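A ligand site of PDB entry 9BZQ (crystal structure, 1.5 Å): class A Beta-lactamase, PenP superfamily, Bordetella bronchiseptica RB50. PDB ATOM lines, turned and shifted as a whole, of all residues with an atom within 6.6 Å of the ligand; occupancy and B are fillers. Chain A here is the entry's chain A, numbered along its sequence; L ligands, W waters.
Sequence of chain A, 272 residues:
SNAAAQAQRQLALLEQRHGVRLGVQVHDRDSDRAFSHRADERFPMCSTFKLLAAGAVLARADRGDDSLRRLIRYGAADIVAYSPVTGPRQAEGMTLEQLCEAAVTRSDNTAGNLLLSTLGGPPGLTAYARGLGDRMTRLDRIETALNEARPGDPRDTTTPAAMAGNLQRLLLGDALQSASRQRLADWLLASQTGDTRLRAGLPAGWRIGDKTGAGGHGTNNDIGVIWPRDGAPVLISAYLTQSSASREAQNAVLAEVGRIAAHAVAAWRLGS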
ATOM      1  N   MET A  45      23.697  21.648 -18.269  1.00  0.00           N
ATOM      2  CA  MET A  45      23.564  23.073 -17.950  1.00  0.00           C
ATOM      3  C   MET A  45      23.566  23.332 -16.448  1.00  0.00           C
ATOM      4  O   MET A  45      24.146  24.328 -15.995  1.00  0.00           O
ATOM      5  CB  MET A  45      22.283  23.641 -18.548  1.00  0.00           C
ATOM      6  CG  MET A  45      22.397  24.013 -20.014  1.00  0.00           C
ATOM      7  SD  MET A  45      20.883  24.792 -20.632  1.00  0.00           S
ATOM      8  CE  MET A  45      19.815  23.356 -20.802  1.00  0.00           C
ATOM      9  N   CYS A  46      22.874  22.493 -15.687  1.00  0.00           N
ATOM     10  CA  CYS A  46      22.577  22.763 -14.286  1.00  0.00           C
ATOM     11  C   CYS A  46      22.038  24.181 -14.151  1.00  0.00           C
ATOM     12  O   CYS A  46      21.215  24.606 -14.985  1.00  0.00           O
ATOM     13  CB  CYS A  46      23.796  22.494 -13.398  1.00  0.00           C
ATOM     14  SG  CYS A  46      24.422  20.807 -13.578  1.00  0.00           S
ATOM     15  N   SER A  47      22.485  24.933 -13.148  1.00  0.00           N
ATOM     16  CA  SER A  47      21.917  26.257 -12.896  1.00  0.00           C
ATOM     17  C   SER A  47      22.126  27.242 -14.031  1.00  0.00           C
ATOM     18  O   SER A  47      21.479  28.296 -14.047  1.00  0.00           O
ATOM     19  CB  SER A  47      22.474  26.876 -11.615  1.00  0.00           C
ATOM     20  OG  SER A  47      21.982  26.290 -10.417  1.00  0.00           O
ATOM     21  N   THR A  48      23.036  26.953 -14.982  1.00  0.00           N
ATOM     22  CA  THR A  48      23.247  27.923 -16.057  1.00  0.00           C
ATOM     23  C   THR A  48      22.017  28.107 -16.941  1.00  0.00           C
ATOM     24  O   THR A  48      21.938  29.119 -17.646  1.00  0.00           O
ATOM     25  CB  THR A  48      24.486  27.606 -16.910  1.00  0.00           C
ATOM     26  OG1 THR A  48      24.279  26.418 -17.682  1.00  0.00           O
ATOM     27  CG2 THR A  48      25.723  27.458 -16.029  1.00  0.00           C
ATOM     28  N   LYS A  50      19.326  29.103 -16.014  1.00  0.00           N
ATOM     29  CA  LYS A  50      18.616  30.253 -15.485  1.00  0.00           C
ATOM     30  C   LYS A  50      18.946  31.524 -16.262  1.00  0.00           C
ATOM     31  O   LYS A  50      18.120  32.437 -16.316  1.00  0.00           O
ATOM     32  CB  LYS A  50      18.912  30.408 -13.999  1.00  0.00           C
ATOM     33  CG  LYS A  50      18.307  29.299 -13.152  1.00  0.00           C
ATOM     34  CD  LYS A  50      18.987  29.140 -11.800  1.00  0.00           C
ATOM     35  CE  LYS A  50      18.435  27.920 -11.062  1.00  0.00           C
ATOM     36  NZ  LYS A  50      19.280  27.502  -9.893  1.00  0.00           N
ATOM     37  N   ALA A  81      15.122  22.506  -3.072  1.00  0.00           N
ATOM     38  CA  ALA A  81      16.408  22.796  -2.470  1.00  0.00           C
ATOM     39  C   ALA A  81      17.069  24.010  -3.106  1.00  0.00           C
ATOM     40  O   ALA A  81      16.889  24.291  -4.295  1.00  0.00           O
ATOM     41  CB  ALA A  81      17.325  21.582  -2.619  1.00  0.00           C
ATOM     42  N   TYR A  82      17.827  24.747  -2.299  1.00  0.00           N
ATOM     43  CA  TYR A  82      18.603  25.913  -2.733  1.00  0.00           C
ATOM     44  C   TYR A  82      17.703  27.021  -3.284  1.00  0.00           C
ATOM     45  O   TYR A  82      17.848  27.485  -4.418  1.00  0.00           O
ATOM     46  CB  TYR A  82      19.706  25.547  -3.745  1.00  0.00           C
ATOM     47  CG  TYR A  82      20.677  24.493  -3.263  1.00  0.00           C
ATOM     48  CD1 TYR A  82      21.677  24.803  -2.350  1.00  0.00           C
ATOM     49  CD2 TYR A  82      20.627  23.196  -3.753  1.00  0.00           C
ATOM     50  CE1 TYR A  82      22.583  23.852  -1.929  1.00  0.00           C
ATOM     51  CE2 TYR A  82      21.529  22.228  -3.343  1.00  0.00           C
ATOM     52  CZ  TYR A  82      22.502  22.564  -2.424  1.00  0.00           C
ATOM     53  OH  TYR A  82      23.414  21.616  -2.010  1.00  0.00           O
ATOM     54  N   ARG A 106      21.159  34.948  -7.465  1.00  0.00           N
ATOM     55  CA  ARG A 106      21.293  34.062  -6.302  1.00  0.00           C
ATOM     56  C   ARG A 106      21.149  32.585  -6.632  1.00  0.00           C
ATOM     57  O   ARG A 106      21.218  31.749  -5.728  1.00  0.00           O
ATOM     58  CB  ARG A 106      20.297  34.455  -5.202  1.00  0.00           C
ATOM     59  CG  ARG A 106      20.425  35.876  -4.687  1.00  0.00           C
ATOM     60  CD  ARG A 106      21.475  36.038  -3.601  1.00  0.00           C
ATOM     61  NE  ARG A 106      21.304  35.100  -2.495  1.00  0.00           N
ATOM     62  CZ  ARG A 106      20.597  35.328  -1.391  1.00  0.00           C
ATOM     63  NH1 ARG A 106      19.890  36.442  -1.234  1.00  0.00           N
ATOM     64  NH2 ARG A 106      20.612  34.430  -0.410  1.00  0.00           N
ATOM     65  N   SER A 107      20.928  32.224  -7.903  1.00  0.00           N
ATOM     66  CA  SER A 107      20.805  30.825  -8.324  1.00  0.00           C
ATOM     67  C   SER A 107      19.625  30.127  -7.667  1.00  0.00           C
ATOM     68  O   SER A 107      19.623  28.905  -7.506  1.00  0.00           O
ATOM     69  CB  SER A 107      22.101  30.028  -8.105  1.00  0.00           C
ATOM     70  OG  SER A 107      22.267  29.067  -9.149  1.00  0.00           O
ATOM     71  N   ASP A 108      18.585  30.884  -7.315  1.00  0.00           N
ATOM     72  CA  ASP A 108      17.444  30.317  -6.592  1.00  0.00           C
ATOM     73  C   ASP A 108      16.722  29.287  -7.466  1.00  0.00           C
ATOM     74  O   ASP A 108      16.303  29.582  -8.593  1.00  0.00           O
ATOM     75  CB  ASP A 108      16.547  31.472  -6.154  1.00  0.00           C
ATOM     76  CG  ASP A 108      15.425  31.047  -5.229  1.00  0.00           C
ATOM     77  OD1 ASP A 108      14.561  30.257  -5.675  1.00  0.00           O
ATOM     78  OD2 ASP A 108      15.383  31.528  -4.071  1.00  0.00           O
ATOM     79  N   ASN A 109      16.587  28.053  -6.943  1.00  0.00           N
ATOM     80  CA  ASN A 109      16.057  26.962  -7.750  1.00  0.00           C
ATOM     81  C   ASN A 109      14.551  27.076  -7.965  1.00  0.00           C
ATOM     82  O   ASN A 109      14.061  26.878  -9.096  1.00  0.00           O
ATOM     83  CB  ASN A 109      16.396  25.612  -7.120  1.00  0.00           C
ATOM     84  CG  ASN A 109      17.738  25.064  -7.579  1.00  0.00           C
ATOM     85  OD1 ASN A 109      18.235  25.419  -8.649  1.00  0.00           O
ATOM     86  ND2 ASN A 109      18.314  24.180  -6.776  1.00  0.00           N
ATOM     87  N   GLU A 143      13.947  21.906 -11.789  1.00  0.00           N
ATOM     88  CA  GLU A 143      14.829  21.780 -10.633  1.00  0.00           C
ATOM     89  C   GLU A 143      14.206  20.852  -9.591  1.00  0.00           C
ATOM     90  O   GLU A 143      12.998  20.914  -9.345  1.00  0.00           O
ATOM     91  CB  GLU A 143      15.058  23.156  -9.991  1.00  0.00           C
ATOM     92  CG  GLU A 143      15.906  24.102 -10.839  1.00  0.00           C
ATOM     93  CD  GLU A 143      17.366  23.723 -10.853  1.00  0.00           C
ATOM     94  OE1 GLU A 143      17.731  22.699 -10.229  1.00  0.00           O
ATOM     95  OE2 GLU A 143      18.148  24.447 -11.487  1.00  0.00           O
ATOM     96  N   THR A 144      15.028  19.993  -8.986  1.00  0.00           N
ATOM     97  CA  THR A 144      16.466  19.832  -9.158  1.00  0.00           C
ATOM     98  C   THR A 144      16.829  18.592  -9.989  1.00  0.00           C
ATOM     99  O   THR A 144      17.997  18.264 -10.131  1.00  0.00           O
ATOM    100  CB  THR A 144      17.198  19.724  -7.810  1.00  0.00           C
ATOM    101  OG1 THR A 144      16.631  18.644  -7.040  1.00  0.00           O
ATOM    102  CG2 THR A 144      17.116  21.035  -7.036  1.00  0.00           C
ATOM    103  N   LEU A 146      17.029  18.242 -13.043  1.00  0.00           N
ATOM    104  CA  LEU A 146      17.856  18.540 -14.213  1.00  0.00           C
ATOM    105  C   LEU A 146      19.349  18.489 -13.923  1.00  0.00           C
ATOM    106  O   LEU A 146      20.137  18.561 -14.862  1.00  0.00           O
ATOM    107  CB  LEU A 146      17.456  19.900 -14.802  1.00  0.00           C
ATOM    108  CG  LEU A 146      17.608  21.149 -13.919  1.00  0.00           C
ATOM    109  CD1 LEU A 146      19.009  21.731 -13.989  1.00  0.00           C
ATOM    110  CD2 LEU A 146      16.605  22.223 -14.308  1.00  0.00           C
ATOM    111  N   ASN A 147      19.762  18.374 -12.658  1.00  0.00           N
ATOM    112  CA  ASN A 147      21.180  18.396 -12.305  1.00  0.00           C
ATOM    113  C   ASN A 147      21.836  17.027 -12.294  1.00  0.00           C
ATOM    114  O   ASN A 147      22.991  16.917 -11.889  1.00  0.00           O
ATOM    115  CB  ASN A 147      21.382  19.062 -10.937  1.00  0.00           C
ATOM    116  CG  ASN A 147      20.853  20.466 -10.895  1.00  0.00           C
ATOM    117  OD1 ASN A 147      21.372  21.349 -11.571  1.00  0.00           O
ATOM    118  ND2 ASN A 147      19.812  20.685 -10.110  1.00  0.00           N
ATOM    119  N   THR A 193      27.887  34.175  -6.565  1.00  0.00           N
ATOM    120  CA  THR A 193      27.984  32.723  -6.513  1.00  0.00           C
ATOM    121  C   THR A 193      29.225  32.180  -7.225  1.00  0.00           C
ATOM    122  O   THR A 193      29.611  31.033  -6.978  1.00  0.00           O
ATOM    123  CB  THR A 193      26.710  32.090  -7.079  1.00  0.00           C
ATOM    124  OG1 THR A 193      26.479  32.578  -8.400  1.00  0.00           O
ATOM    125  CG2 THR A 193      25.504  32.431  -6.218  1.00  0.00           C
ATOM    126  N   GLY A 194      29.829  32.973  -8.110  1.00  0.00           N
ATOM    127  CA  GLY A 194      31.036  32.571  -8.802  1.00  0.00           C
ATOM    128  C   GLY A 194      32.305  33.247  -8.338  1.00  0.00           C
ATOM    129  O   GLY A 194      33.286  33.296  -9.086  1.00  0.00           O
ATOM    130  N   ARG A 197      35.202  31.069  -8.845  1.00  0.00           N
ATOM    131  CA  ARG A 197      35.253  30.445 -10.160  1.00  0.00           C
ATOM    132  C   ARG A 197      35.878  31.423 -11.149  1.00  0.00           C
ATOM    133  O   ARG A 197      36.956  31.942 -10.844  1.00  0.00           O
ATOM    134  CB  ARG A 197      33.892  29.828 -10.515  1.00  0.00           C
ATOM    135  CG  ARG A 197      33.639  28.572  -9.676  1.00  0.00           C
ATOM    136  CD  ARG A 197      32.260  27.947  -9.863  1.00  0.00           C
ATOM    137  NE  ARG A 197      31.305  28.365  -8.853  1.00  0.00           N
ATOM    138  CZ  ARG A 197      30.105  27.819  -8.703  1.00  0.00           C
ATOM    139  NH1 ARG A 197      29.719  26.794  -9.455  1.00  0.00           N
ATOM    140  NH2 ARG A 197      29.272  28.313  -7.794  1.00  0.00           N
ATOM    141  N   LYS A 211      26.904  33.387 -14.685  1.00  0.00           N
ATOM    142  CA  LYS A 211      25.945  32.467 -14.100  1.00  0.00           C
ATOM    143  C   LYS A 211      26.638  31.134 -13.859  1.00  0.00           C
ATOM    144  O   LYS A 211      27.072  30.473 -14.802  1.00  0.00           O
ATOM    145  CB  LYS A 211      24.713  32.267 -14.990  1.00  0.00           C
ATOM    146  CG  LYS A 211      23.677  31.347 -14.340  1.00  0.00           C
ATOM    147  CD  LYS A 211      22.935  32.039 -13.190  1.00  0.00           C
ATOM    148  CE  LYS A 211      22.430  31.045 -12.163  1.00  0.00           C
ATOM    149  NZ  LYS A 211      23.509  30.511 -11.268  1.00  0.00           N
ATOM    150  N   THR A 212      26.741  30.755 -12.587  1.00  0.00           N
ATOM    151  CA  THR A 212      27.354  29.510 -12.174  1.00  0.00           C
ATOM    152  C   THR A 212      26.378  28.343 -12.265  1.00  0.00           C
ATOM    153  O   THR A 212      25.160  28.518 -12.432  1.00  0.00           O
ATOM    154  CB  THR A 212      27.815  29.626 -10.722  1.00  0.00           C
ATOM    155  OG1 THR A 212      26.781  30.253  -9.968  1.00  0.00           O
ATOM    156  CG2 THR A 212      29.103  30.440 -10.625  1.00  0.00           C
ATOM    157  N   GLY A 213      26.915  27.139 -12.150  1.00  0.00           N
ATOM    158  CA  GLY A 213      26.098  25.957 -11.938  1.00  0.00           C
ATOM    159  C   GLY A 213      26.926  24.832 -11.354  1.00  0.00           C
ATOM    160  O   GLY A 213      28.155  24.865 -11.380  1.00  0.00           O
ATOM    161  N   ALA A 214      26.224  23.834 -10.811  1.00  0.00           N
ATOM    162  CA  ALA A 214      26.885  22.660 -10.263  1.00  0.00           C
ATOM    163  C   ALA A 214      25.894  21.504 -10.254  1.00  0.00           C
ATOM    164  O   ALA A 214      24.690  21.707 -10.040  1.00  0.00           O
ATOM    165  CB  ALA A 214      27.404  22.912  -8.835  1.00  0.00           C
ATOM    166  N   GLY A 215      26.396  20.297 -10.495  1.00  0.00           N
ATOM    167  CA  GLY A 215      25.522  19.136 -10.537  1.00  0.00           C
ATOM    168  C   GLY A 215      26.208  17.834 -10.193  1.00  0.00           C
ATOM    169  O   GLY A 215      27.327  17.825  -9.671  1.00  0.00           O
ATOM    170  N   ASN A 220      30.489  21.259 -12.765  1.00  0.00           N
ATOM    171  CA  ASN A 220      30.644  22.591 -12.196  1.00  0.00           C
ATOM    172  C   ASN A 220      30.881  23.538 -13.357  1.00  0.00           C
ATOM    173  O   ASN A 220      31.784  23.314 -14.163  1.00  0.00           O
ATOM    174  CB  ASN A 220      31.846  22.590 -11.229  1.00  0.00           C
ATOM    175  CG  ASN A 220      31.805  23.728 -10.260  1.00  0.00           C
ATOM    176  OD1 ASN A 220      31.442  24.839 -10.628  1.00  0.00           O
ATOM    177  ND2 ASN A 220      32.179  23.475  -9.013  1.00  0.00           N
ATOM    178  N   ASN A 221      30.039  24.584 -13.461  1.00  0.00           N
ATOM    179  CA  ASN A 221      29.989  25.413 -14.659  1.00  0.00           C
ATOM    180  C   ASN A 221      30.038  26.894 -14.302  1.00  0.00           C
ATOM    181  O   ASN A 221      29.659  27.299 -13.209  1.00  0.00           O
ATOM    182  CB  ASN A 221      28.661  25.186 -15.418  1.00  0.00           C
ATOM    183  CG  ASN A 221      28.398  23.729 -15.703  1.00  0.00           C
ATOM    184  OD1 ASN A 221      29.315  22.950 -15.941  1.00  0.00           O
ATOM    185  ND2 ASN A 221      27.114  23.343 -15.692  1.00  0.00           N
ATOM    186  N   ARG A 247      34.320  20.143  -4.379  1.00  0.00           N
ATOM    187  CA  ARG A 247      33.780  21.327  -5.021  1.00  0.00           C
ATOM    188  C   ARG A 247      34.805  22.452  -5.088  1.00  0.00           C
ATOM    189  O   ARG A 247      34.906  23.149  -6.098  1.00  0.00           O
ATOM    190  CB  ARG A 247      32.522  21.809  -4.286  1.00  0.00           C
ATOM    191  CG  ARG A 247      31.327  20.878  -4.402  1.00  0.00           C
ATOM    192  CD  ARG A 247      30.939  20.657  -5.867  1.00  0.00           C
ATOM    193  NE  ARG A 247      29.650  20.010  -6.014  1.00  0.00           N
ATOM    194  CZ  ARG A 247      29.137  19.645  -7.178  1.00  0.00           C
ATOM    195  NH1 ARG A 247      29.829  19.748  -8.301  1.00  0.00           N
ATOM    196  NH2 ARG A 247      27.891  19.166  -7.225  1.00  0.00           N
HETATM  197  O1  LIG L   1      23.486  24.621 -10.667  1.00  0.00           O
HETATM  198  C1  LIG L   1      22.812  25.322  -9.926  1.00  0.00           C
HETATM  199  N1  LIG L   1      22.531  25.025  -8.647  1.00  0.00           N
HETATM  200  C2  LIG L   1      21.800  25.924  -7.743  1.00  0.00           C
HETATM  201  C3  LIG L   1      22.953  23.741  -8.072  1.00  0.00           C
HETATM  202  C4  LIG L   1      21.737  22.869  -7.751  1.00  0.00           C
HETATM  203  O2  LIG L   1      20.630  23.137  -8.190  1.00  0.00           O
HETATM  204  N2  LIG L   1      21.931  21.705  -6.908  1.00  0.00           N
HETATM  205  C5  LIG L   1      23.838  24.001  -6.857  1.00  0.00           C
HETATM  206  C6  LIG L   1      23.160  24.929  -5.848  1.00  0.00           C
HETATM  207  C7  LIG L   1      22.640  26.227  -6.485  1.00  0.00           C
HETATM  208  N3  LIG L   1      23.688  27.249  -6.719  1.00  0.00           N
HETATM  209  O3  LIG L   1      24.930  26.663  -7.161  1.00  0.00           O
HETATM  210  S1  LIG L   1      25.550  27.437  -8.374  1.00  0.00           S
HETATM  211  O4  LIG L   1      26.683  26.627  -8.752  1.00  0.00           O
HETATM  212  O5  LIG L   1      24.529  27.513  -9.387  1.00  0.00           O
HETATM  213  O6  LIG L   1      25.929  28.751  -7.893  1.00  0.00           O
HETATM  214  O   HOH W   1      24.657  19.871  -7.287  1.00  0.00           O
HETATM  215  O   HOH W   2      20.541  23.776 -10.946  1.00  0.00           O
HETATM  216  O   HOH W   3      24.310  27.779  -3.721  1.00  0.00           O
HETATM  217  O   HOH W   4      26.753  28.916  -5.170  1.00  0.00           O
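An oxygen (O1) of the ligand sits close to the backbone NH of Ser 47, at 2.7 Å.
The side-chain hydroxyl of Ser 47 is covalently linked to a carbon (C1) of the ligand.
O6 of the ligand is in hydrogen-bond range of OG1 of Thr 212, at 2.7 Å.
O5 of the ligand lies within hydrogen-bond range of OG of Ser 107, at 2.8 Å.
The backbone NH of Ala 214 lies within hydrogen-bond range of an oxygen (O1) of the ligand (2.9 Å).
O2 of the ligand is in hydrogen-bond range of ND2 of Asn 109.
The guanidinium group (NH1) of Arg 197 is in salt-bridge range of an oxygen (O4) of the ligand (3.1 Å).
N of Gly 213 sits close to O4 of the ligand, at 3.4 Å.
The side-chain amide nitrogen (ND2) of Asn 147 lies within hydrogen-bond range of an oxygen (O2) of the ligand (3.2 Å).
The side-chain amino group (NZ) of Lys 211 is in salt-bridge range of an oxygen (O5) of the ligand (3.7 Å).
The side-chain hydroxyl of Ser 47 is in hydrogen-bond range of the side-chain hydroxyl of Ser 107, 3.1 Å away.
The side-chain amide oxygen (OD1) of Asn 109 lies close to the side-chain carboxylate (OE2) of Glu 143, at 3.0 Å.
N of Asn 109 lies within hydrogen-bond range of O of Tyr 82 (2.9 Å).
ND2 of Asn 109 sits at hydrogen-bond distance from O of Ala 81 (2.9 Å).
The backbone carbonyl oxygen of Thr 193 lies within hydrogen-bond range of the guanidinium group of Arg 197.
The guanidinium group (NH1) of Arg 197 lies within hydrogen-bond range of the side-chain amide oxygen (OD1) of Asn 220 (2.9 Å).
ND2 of Asn 147 lies within hydrogen-bond range of OE1 of Glu 143, at 2.9 Å.
The side-chain sulfur (SG) of Cys 46 sits close to the backbone NH (N) of Gly 215 (3.7 Å).
Residues that only touch the ligand: Cys 46 (3.5 Å), Lys 50 (3.7 Å), Tyr 82 (3.6 Å), Glu 143 (3.6 Å) and Thr 193 (3.5 Å).
Hydrophobic or aromatic side chains within 4 Å of the ligand: Tyr 82 and Ala 214.
14 residues have an atom within 4 Å of the ligand: Cys 46, Ser 47, Lys 50, Tyr 82, Ser 107, Asn 109, Glu 143, Asn 147, Thr 193, Arg 197, Lys 211, Thr 212, Gly 213 and Ala 214.
Water W1 lies within hydrogen-bond range of a nitrogen (N2) of the ligand, the backbone carbonyl oxygen of Ala 214 and the guanidinium group of Arg 247.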
